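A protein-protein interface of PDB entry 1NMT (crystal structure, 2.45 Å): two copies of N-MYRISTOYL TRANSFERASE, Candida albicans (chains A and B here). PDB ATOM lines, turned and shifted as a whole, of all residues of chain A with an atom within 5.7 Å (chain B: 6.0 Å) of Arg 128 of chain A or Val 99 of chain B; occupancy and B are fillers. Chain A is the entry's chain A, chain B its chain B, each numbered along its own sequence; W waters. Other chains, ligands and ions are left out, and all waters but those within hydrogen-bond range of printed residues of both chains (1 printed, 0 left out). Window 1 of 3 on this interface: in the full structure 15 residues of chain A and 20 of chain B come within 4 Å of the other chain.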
ATOM      1  N   LEU A 124      12.719  20.408   9.081  1.00  0.00           N
ATOM      2  CA  LEU A 124      12.265  19.813  10.329  1.00  0.00           C
ATOM      3  C   LEU A 124      11.165  20.626  11.008  1.00  0.00           C
ATOM      4  O   LEU A 124      10.867  20.404  12.188  1.00  0.00           O
ATOM      5  CB  LEU A 124      13.441  19.654  11.266  1.00  0.00           C
ATOM      6  CG  LEU A 124      14.621  18.932  10.640  1.00  0.00           C
ATOM      7  CD1 LEU A 124      15.596  18.578  11.721  1.00  0.00           C
ATOM      8  CD2 LEU A 124      14.148  17.661   9.938  1.00  0.00           C
ATOM      9  N   ARG A 125      10.564  21.558  10.263  1.00  0.00           N
ATOM     10  CA  ARG A 125       9.506  22.412  10.804  1.00  0.00           C
ATOM     11  C   ARG A 125       8.346  21.564  11.294  1.00  0.00           C
ATOM     12  O   ARG A 125       7.535  22.006  12.102  1.00  0.00           O
ATOM     13  CB  ARG A 125       9.025  23.406   9.736  1.00  0.00           C
ATOM     14  CG  ARG A 125      10.029  24.536   9.430  1.00  0.00           C
ATOM     15  CD  ARG A 125      10.776  24.968  10.704  1.00  0.00           C
ATOM     16  NE  ARG A 125      11.837  25.969  10.512  1.00  0.00           N
ATOM     17  CZ  ARG A 125      11.797  26.989   9.654  1.00  0.00           C
ATOM     18  NH1 ARG A 125      10.738  27.180   8.865  1.00  0.00           N
ATOM     19  NH2 ARG A 125      12.814  27.845   9.608  1.00  0.00           N
ATOM     20  N   ASN A 126       8.309  20.326  10.832  1.00  0.00           N
ATOM     21  CA  ASN A 126       7.250  19.408  11.200  1.00  0.00           C
ATOM     22  C   ASN A 126       7.669  18.390  12.260  1.00  0.00           C
ATOM     23  O   ASN A 126       6.971  17.399  12.463  1.00  0.00           O
ATOM     24  CB  ASN A 126       6.731  18.658   9.957  1.00  0.00           C
ATOM     25  CG  ASN A 126       5.932  19.566   8.985  1.00  0.00           C
ATOM     26  OD1 ASN A 126       5.404  20.630   9.366  1.00  0.00           O
ATOM     27  ND2 ASN A 126       5.843  19.131   7.720  1.00  0.00           N
ATOM     28  N   LYS A 127       8.801  18.606  12.925  1.00  0.00           N
ATOM     29  CA  LYS A 127       9.219  17.672  13.970  1.00  0.00           C
ATOM     30  C   LYS A 127       8.824  18.277  15.328  1.00  0.00           C
ATOM     31  O   LYS A 127       8.929  17.615  16.370  1.00  0.00           O
ATOM     32  CB  LYS A 127      10.741  17.402  13.909  1.00  0.00           C
ATOM     33  CG  LYS A 127      11.211  16.597  12.695  1.00  0.00           C
ATOM     34  CD  LYS A 127      10.691  15.184  12.771  1.00  0.00           C
ATOM     35  CE  LYS A 127      11.094  14.310  11.574  1.00  0.00           C
ATOM     36  NZ  LYS A 127      11.207  12.867  12.045  1.00  0.00           N
ATOM     37  N   ARG A 128       8.371  19.537  15.302  1.00  0.00           N
ATOM     38  CA  ARG A 128       7.913  20.265  16.494  1.00  0.00           C
ATOM     39  C   ARG A 128       8.986  20.323  17.562  1.00  0.00           C
ATOM     40  O   ARG A 128       8.795  19.905  18.713  1.00  0.00           O
ATOM     41  CB  ARG A 128       6.660  19.622  17.072  1.00  0.00           C
ATOM     42  CG  ARG A 128       5.375  19.970  16.299  1.00  0.00           C
ATOM     43  CD  ARG A 128       4.459  18.763  16.245  1.00  0.00           C
ATOM     44  NE  ARG A 128       3.296  18.958  17.076  1.00  0.00           N
ATOM     45  CZ  ARG A 128       2.666  18.006  17.749  1.00  0.00           C
ATOM     46  NH1 ARG A 128       3.074  16.751  17.714  1.00  0.00           N
ATOM     47  NH2 ARG A 128       1.610  18.329  18.476  1.00  0.00           N
ATOM     48  N   LEU A 129      10.109  20.882  17.150  1.00  0.00           N
ATOM     49  CA  LEU A 129      11.274  21.026  17.993  1.00  0.00           C
ATOM     50  C   LEU A 129      11.359  22.249  18.887  1.00  0.00           C
ATOM     51  O   LEU A 129      11.985  22.148  19.942  1.00  0.00           O
ATOM     52  CB  LEU A 129      12.523  20.990  17.120  1.00  0.00           C
ATOM     53  CG  LEU A 129      12.812  19.634  16.463  1.00  0.00           C
ATOM     54  CD1 LEU A 129      13.915  19.760  15.375  1.00  0.00           C
ATOM     55  CD2 LEU A 129      13.255  18.673  17.557  1.00  0.00           C
ATOM     56  N   ALA A 130      10.774  23.383  18.477  1.00  0.00           N
ATOM     57  CA  ALA A 130      10.855  24.602  19.290  1.00  0.00           C
ATOM     58  C   ALA A 130      10.567  24.323  20.769  1.00  0.00           C
ATOM     59  O   ALA A 130      11.420  24.547  21.622  1.00  0.00           O
ATOM     60  CB  ALA A 130       9.886  25.691  18.756  1.00  0.00           C
ATOM     61  N   PRO A 131       9.365  23.812  21.094  1.00  0.00           N
ATOM     62  CA  PRO A 131       9.104  23.560  22.518  1.00  0.00           C
ATOM     63  C   PRO A 131      10.194  22.761  23.219  1.00  0.00           C
ATOM     64  O   PRO A 131      10.461  22.962  24.411  1.00  0.00           O
ATOM     65  CB  PRO A 131       7.763  22.822  22.539  1.00  0.00           C
ATOM     66  CG  PRO A 131       7.335  22.659  21.131  1.00  0.00           C
ATOM     67  CD  PRO A 131       8.222  23.465  20.233  1.00  0.00           C
ATOM     68  N   VAL A 132      10.829  21.857  22.484  1.00  0.00           N
ATOM     69  CA  VAL A 132      11.875  21.000  23.060  1.00  0.00           C
ATOM     70  C   VAL A 132      13.180  21.768  23.303  1.00  0.00           C
ATOM     71  O   VAL A 132      13.915  21.509  24.276  1.00  0.00           O
ATOM     72  CB  VAL A 132      12.173  19.798  22.137  1.00  0.00           C
ATOM     73  CG1 VAL A 132      13.145  18.844  22.821  1.00  0.00           C
ATOM     74  CG2 VAL A 132      10.877  19.068  21.783  1.00  0.00           C
ATOM     75  N   TRP B  78       1.358   7.561  10.753  1.00  0.00           N
ATOM     76  CA  TRP B  78       0.367   7.546  11.817  1.00  0.00           C
ATOM     77  C   TRP B  78      -1.035   7.164  11.339  1.00  0.00           C
ATOM     78  O   TRP B  78      -2.024   7.337  12.055  1.00  0.00           O
ATOM     79  CB  TRP B  78       0.356   8.909  12.517  1.00  0.00           C
ATOM     80  CG  TRP B  78       1.564   9.126  13.393  1.00  0.00           C
ATOM     81  CD1 TRP B  78       2.514   8.199  13.727  1.00  0.00           C
ATOM     82  CD2 TRP B  78       1.919  10.330  14.094  1.00  0.00           C
ATOM     83  NE1 TRP B  78       3.431   8.748  14.592  1.00  0.00           N
ATOM     84  CE2 TRP B  78       3.090  10.052  14.837  1.00  0.00           C
ATOM     85  CE3 TRP B  78       1.359  11.620  14.168  1.00  0.00           C
ATOM     86  CZ2 TRP B  78       3.715  11.021  15.653  1.00  0.00           C
ATOM     87  CZ3 TRP B  78       1.983  12.584  14.975  1.00  0.00           C
ATOM     88  CH2 TRP B  78       3.150  12.274  15.707  1.00  0.00           C
ATOM     89  N   THR B  97      -3.220  12.392  14.792  1.00  0.00           N
ATOM     90  CA  THR B  97      -3.033  13.694  14.144  1.00  0.00           C
ATOM     91  C   THR B  97      -2.414  14.614  15.215  1.00  0.00           C
ATOM     92  O   THR B  97      -2.882  14.647  16.357  1.00  0.00           O
ATOM     93  CB  THR B  97      -4.407  14.268  13.655  1.00  0.00           C
ATOM     94  OG1 THR B  97      -5.064  13.310  12.805  1.00  0.00           O
ATOM     95  CG2 THR B  97      -4.209  15.543  12.833  1.00  0.00           C
ATOM     96  N   PRO B  98      -1.361  15.364  14.870  1.00  0.00           N
ATOM     97  CA  PRO B  98      -0.707  16.262  15.846  1.00  0.00           C
ATOM     98  C   PRO B  98      -1.589  17.379  16.368  1.00  0.00           C
ATOM     99  O   PRO B  98      -2.350  17.962  15.609  1.00  0.00           O
ATOM    100  CB  PRO B  98       0.501  16.836  15.093  1.00  0.00           C
ATOM    101  CG  PRO B  98       0.210  16.600  13.630  1.00  0.00           C
ATOM    102  CD  PRO B  98      -0.747  15.430  13.531  1.00  0.00           C
ATOM    103  N   VAL B  99      -1.469  17.685  17.657  1.00  0.00           N
ATOM    104  CA  VAL B  99      -2.251  18.755  18.261  1.00  0.00           C
ATOM    105  C   VAL B  99      -1.478  19.244  19.500  1.00  0.00           C
ATOM    106  O   VAL B  99      -0.693  18.479  20.084  1.00  0.00           O
ATOM    107  CB  VAL B  99      -3.664  18.227  18.678  1.00  0.00           C
ATOM    108  CG1 VAL B  99      -3.536  17.043  19.634  1.00  0.00           C
ATOM    109  CG2 VAL B  99      -4.446  19.295  19.381  1.00  0.00           C
ATOM    110  N   THR B 100      -1.675  20.508  19.883  1.00  0.00           N
ATOM    111  CA  THR B 100      -1.037  21.059  21.094  1.00  0.00           C
ATOM    112  C   THR B 100      -2.131  21.456  22.083  1.00  0.00           C
ATOM    113  O   THR B 100      -3.031  22.195  21.719  1.00  0.00           O
ATOM    114  CB  THR B 100      -0.225  22.337  20.786  1.00  0.00           C
ATOM    115  OG1 THR B 100       0.770  22.055  19.784  1.00  0.00           O
ATOM    116  CG2 THR B 100       0.439  22.858  22.068  1.00  0.00           C
ATOM    117  N   PHE B 101      -2.062  20.994  23.323  1.00  0.00           N
ATOM    118  CA  PHE B 101      -3.073  21.340  24.334  1.00  0.00           C
ATOM    119  C   PHE B 101      -2.402  22.196  25.406  1.00  0.00           C
ATOM    120  O   PHE B 101      -1.160  22.225  25.525  1.00  0.00           O
ATOM    121  CB  PHE B 101      -3.573  20.091  25.075  1.00  0.00           C
ATOM    122  CG  PHE B 101      -4.216  19.083  24.211  1.00  0.00           C
ATOM    123  CD1 PHE B 101      -5.368  19.398  23.482  1.00  0.00           C
ATOM    124  CD2 PHE B 101      -3.713  17.786  24.148  1.00  0.00           C
ATOM    125  CE1 PHE B 101      -6.025  18.419  22.695  1.00  0.00           C
ATOM    126  CE2 PHE B 101      -4.359  16.795  23.364  1.00  0.00           C
ATOM    127  CZ  PHE B 101      -5.516  17.116  22.639  1.00  0.00           C
ATOM    128  N   ILE B 110       1.326  21.116  26.319  1.00  0.00           N
ATOM    129  CA  ILE B 110       1.791  19.804  25.925  1.00  0.00           C
ATOM    130  C   ILE B 110       1.569  19.468  24.443  1.00  0.00           C
ATOM    131  O   ILE B 110       0.423  19.465  23.933  1.00  0.00           O
ATOM    132  CB  ILE B 110       1.116  18.719  26.796  1.00  0.00           C
ATOM    133  CG1 ILE B 110       1.343  19.011  28.274  1.00  0.00           C
ATOM    134  CG2 ILE B 110       1.679  17.357  26.461  1.00  0.00           C
ATOM    135  CD1 ILE B 110       0.257  18.378  29.150  1.00  0.00           C
ATOM    136  N   ASP B 111       2.666  19.206  23.744  1.00  0.00           N
ATOM    137  CA  ASP B 111       2.581  18.792  22.343  1.00  0.00           C
ATOM    138  C   ASP B 111       2.125  17.314  22.368  1.00  0.00           C
ATOM    139  O   ASP B 111       2.776  16.448  22.954  1.00  0.00           O
ATOM    140  CB  ASP B 111       3.936  18.944  21.645  1.00  0.00           C
ATOM    141  CG  ASP B 111       4.039  20.265  20.860  1.00  0.00           C
ATOM    142  OD1 ASP B 111       3.063  21.064  20.902  1.00  0.00           O
ATOM    143  OD2 ASP B 111       5.081  20.519  20.203  1.00  0.00           O
ATOM    144  N   SER B 112       0.978  17.052  21.760  1.00  0.00           N
ATOM    145  CA  SER B 112       0.404  15.720  21.777  1.00  0.00           C
ATOM    146  C   SER B 112      -0.136  15.322  20.451  1.00  0.00           C
ATOM    147  O   SER B 112       0.270  15.794  19.387  1.00  0.00           O
ATOM    148  CB  SER B 112      -0.751  15.595  22.786  1.00  0.00           C
ATOM    149  OG  SER B 112      -0.507  16.404  23.920  1.00  0.00           O
ATOM    150  N   VAL B 113      -1.143  14.489  20.544  1.00  0.00           N
ATOM    151  CA  VAL B 113      -1.732  13.957  19.365  1.00  0.00           C
ATOM    152  C   VAL B 113      -3.171  13.613  19.691  1.00  0.00           C
ATOM    153  O   VAL B 113      -3.527  13.371  20.851  1.00  0.00           O
ATOM    154  CB  VAL B 113      -0.865  12.710  18.993  1.00  0.00           C
ATOM    155  CG1 VAL B 113      -1.571  11.426  19.360  1.00  0.00           C
ATOM    156  CG2 VAL B 113      -0.425  12.797  17.584  1.00  0.00           C
ATOM    157  N   GLU B 114      -4.020  13.637  18.677  1.00  0.00           N
ATOM    158  CA  GLU B 114      -5.398  13.222  18.897  1.00  0.00           C
ATOM    159  C   GLU B 114      -5.558  11.873  18.190  1.00  0.00           C
ATOM    160  O   GLU B 114      -5.169  11.714  17.028  1.00  0.00           O
ATOM    161  CB  GLU B 114      -6.385  14.224  18.329  1.00  0.00           C
ATOM    162  CG  GLU B 114      -7.799  13.764  18.571  1.00  0.00           C
ATOM    163  CD  GLU B 114      -8.809  14.442  17.671  1.00  0.00           C
ATOM    164  OE1 GLU B 114      -8.455  15.484  17.058  1.00  0.00           O
ATOM    165  OE2 GLU B 114      -9.950  13.915  17.586  1.00  0.00           O
ATOM    166  N   ILE B 146       6.476  11.901  21.525  1.00  0.00           N
ATOM    167  CA  ILE B 146       5.229  12.517  21.980  1.00  0.00           C
ATOM    168  C   ILE B 146       4.749  11.507  23.002  1.00  0.00           C
ATOM    169  O   ILE B 146       4.705  10.314  22.699  1.00  0.00           O
ATOM    170  CB  ILE B 146       4.202  12.692  20.838  1.00  0.00           C
ATOM    171  CG1 ILE B 146       4.777  13.618  19.770  1.00  0.00           C
ATOM    172  CG2 ILE B 146       2.919  13.357  21.358  1.00  0.00           C
ATOM    173  CD1 ILE B 146       4.967  15.054  20.239  1.00  0.00           C
ATOM    174  N   LEU B 150      -4.772  12.374  23.216  1.00  0.00           N
ATOM    175  CA  LEU B 150      -6.161  12.580  23.544  1.00  0.00           C
ATOM    176  C   LEU B 150      -6.962  11.605  22.725  1.00  0.00           C
ATOM    177  O   LEU B 150      -6.699  11.450  21.537  1.00  0.00           O
ATOM    178  CB  LEU B 150      -6.594  13.984  23.183  1.00  0.00           C
ATOM    179  CG  LEU B 150      -8.017  14.200  23.699  1.00  0.00           C
ATOM    180  CD1 LEU B 150      -7.958  14.556  25.207  1.00  0.00           C
ATOM    181  CD2 LEU B 150      -8.711  15.280  22.892  1.00  0.00           C
ATOM    182  N   GLN B 234      -6.809  24.268  23.224  1.00  0.00           N
ATOM    183  CA  GLN B 234      -5.886  23.957  22.152  1.00  0.00           C
ATOM    184  C   GLN B 234      -5.113  25.204  21.743  1.00  0.00           C
ATOM    185  O   GLN B 234      -5.665  26.307  21.730  1.00  0.00           O
ATOM    186  CB  GLN B 234      -6.680  23.441  20.944  1.00  0.00           C
ATOM    187  CG  GLN B 234      -5.864  22.681  19.949  1.00  0.00           C
ATOM    188  CD  GLN B 234      -6.703  22.107  18.813  1.00  0.00           C
ATOM    189  OE1 GLN B 234      -7.922  21.879  18.949  1.00  0.00           O
ATOM    190  NE2 GLN B 234      -6.057  21.878  17.684  1.00  0.00           N
ATOM    191  N   LEU B 235      -3.839  25.039  21.403  1.00  0.00           N
ATOM    192  CA  LEU B 235      -3.032  26.168  20.920  1.00  0.00           C
ATOM    193  C   LEU B 235      -2.684  25.852  19.461  1.00  0.00           C
ATOM    194  O   LEU B 235      -2.518  24.686  19.097  1.00  0.00           O
ATOM    195  CB  LEU B 235      -1.751  26.312  21.746  1.00  0.00           C
ATOM    196  CG  LEU B 235      -1.655  27.258  22.958  1.00  0.00           C
ATOM    197  CD1 LEU B 235      -2.997  27.442  23.650  1.00  0.00           C
ATOM    198  CD2 LEU B 235      -0.640  26.717  23.923  1.00  0.00           C
ATOM    199  N   GLU B 240      -1.519  26.369  11.462  1.00  0.00           N
ATOM    200  CA  GLU B 240      -2.497  25.372  11.894  1.00  0.00           C
ATOM    201  C   GLU B 240      -3.895  25.984  12.006  1.00  0.00           C
ATOM    202  O   GLU B 240      -4.873  25.388  11.546  1.00  0.00           O
ATOM    203  CB  GLU B 240      -2.123  24.758  13.261  1.00  0.00           C
ATOM    204  CG  GLU B 240      -0.855  23.947  13.235  1.00  0.00           C
ATOM    205  CD  GLU B 240      -0.367  23.519  14.613  1.00  0.00           C
ATOM    206  OE1 GLU B 240      -0.599  24.246  15.611  1.00  0.00           O
ATOM    207  OE2 GLU B 240       0.268  22.441  14.692  1.00  0.00           O
HETATM  208  O   HOH W   1       7.355  19.042  20.517  1.00  0.00           O
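NH2 of Arg 128 of chain A sits at hydrogen-bond distance from O of Val 99 of chain B (2.8 Å).
NE of Arg 128 of chain A is in salt-bridge range of OD2 of Asp 111 of chain B, 3.9 Å away.
The guanidinium group of Arg 128 of chain A is in hydrogen-bond range of the backbone carbonyl oxygen of Ser 112 of chain B.
The backbone NH of Ser 112 of chain B lies within hydrogen-bond range of the backbone carbonyl oxygen of Val 99 of chain B (2.8 Å).
OG1 of Thr 100 of chain B is in hydrogen-bond range of OD1 of Asp 111 of chain B (2.7 Å).
The side-chain hydroxyl (OG) of Ser 112 of chain B is in hydrogen-bond range of the backbone carbonyl oxygen (O) of Ile 110 of chain B, 3.2 Å away.
CZ of Arg 128 of chain A touches CB of Pro 98 of chain B (3.6 Å).
Arg 128 of chain A touches Ile 146 of chain B (NH1 to CD1, 3.6 Å).
Asp 111 of chain B touches Pro 131 of chain A.
Arg 128 of chain A touches just these residues of chain B: Pro 98, Val 99, Asp 111, Ser 112 and Ile 146.
Printed residues of chain A within 4 Å of Pro 98 of chain B: Arg 128 (3.6 Å).
Printed residues of chain A within 4 Å of Ser 112 of chain B: Arg 128.
Of the printed residues of chain A, Ile 146 of chain B touches Arg 128 (3.6 Å).
Of the printed residues of chain A, Asp 111 of chain B touches Arg 128 (3.6 Å) and Pro 131 (3.2 Å).
Of the printed residues of chain B, Pro 131 of chain A touches Asp 111 (3.2 Å).
Lys 127 of chain A touches none of the printed residues of chain B.
Trp 78 of chain B touches none of the printed residues of chain A.
The nearest printed residue of chain A that does not touch Val 99 of chain B is Pro 131 of chain A (9.1 Å).
The nearest printed residue of chain B that does not touch Pro 131 of chain A is Thr 100 of chain B (6.7 Å).
Of the 16 printed residues of chain B, 5 touch a printed residue of chain A.
Hydrophobic or aromatic side chains of chain B within 4 Å of the printed part of chain A: Pro 98 and Ile 146.
Among the printed residues, 6 pairs touch across the chains.
Among the printed residues, Asp or Glu carboxylates within 4 Å of a Lys or Arg side-chain nitrogen of the other chain: Arg 128 of chain A with Asp 111 of chain B.
No position is printed for both chains.
Of the 6 pairs that touch across the chains among the printed residues, none has its exchanged pair printed and touching as well.
Water W1 lies within hydrogen-bond range of O of Arg 128 of chain A (2.5 Å) and OD2 of Asp 111 of chain B (2.7 Å).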
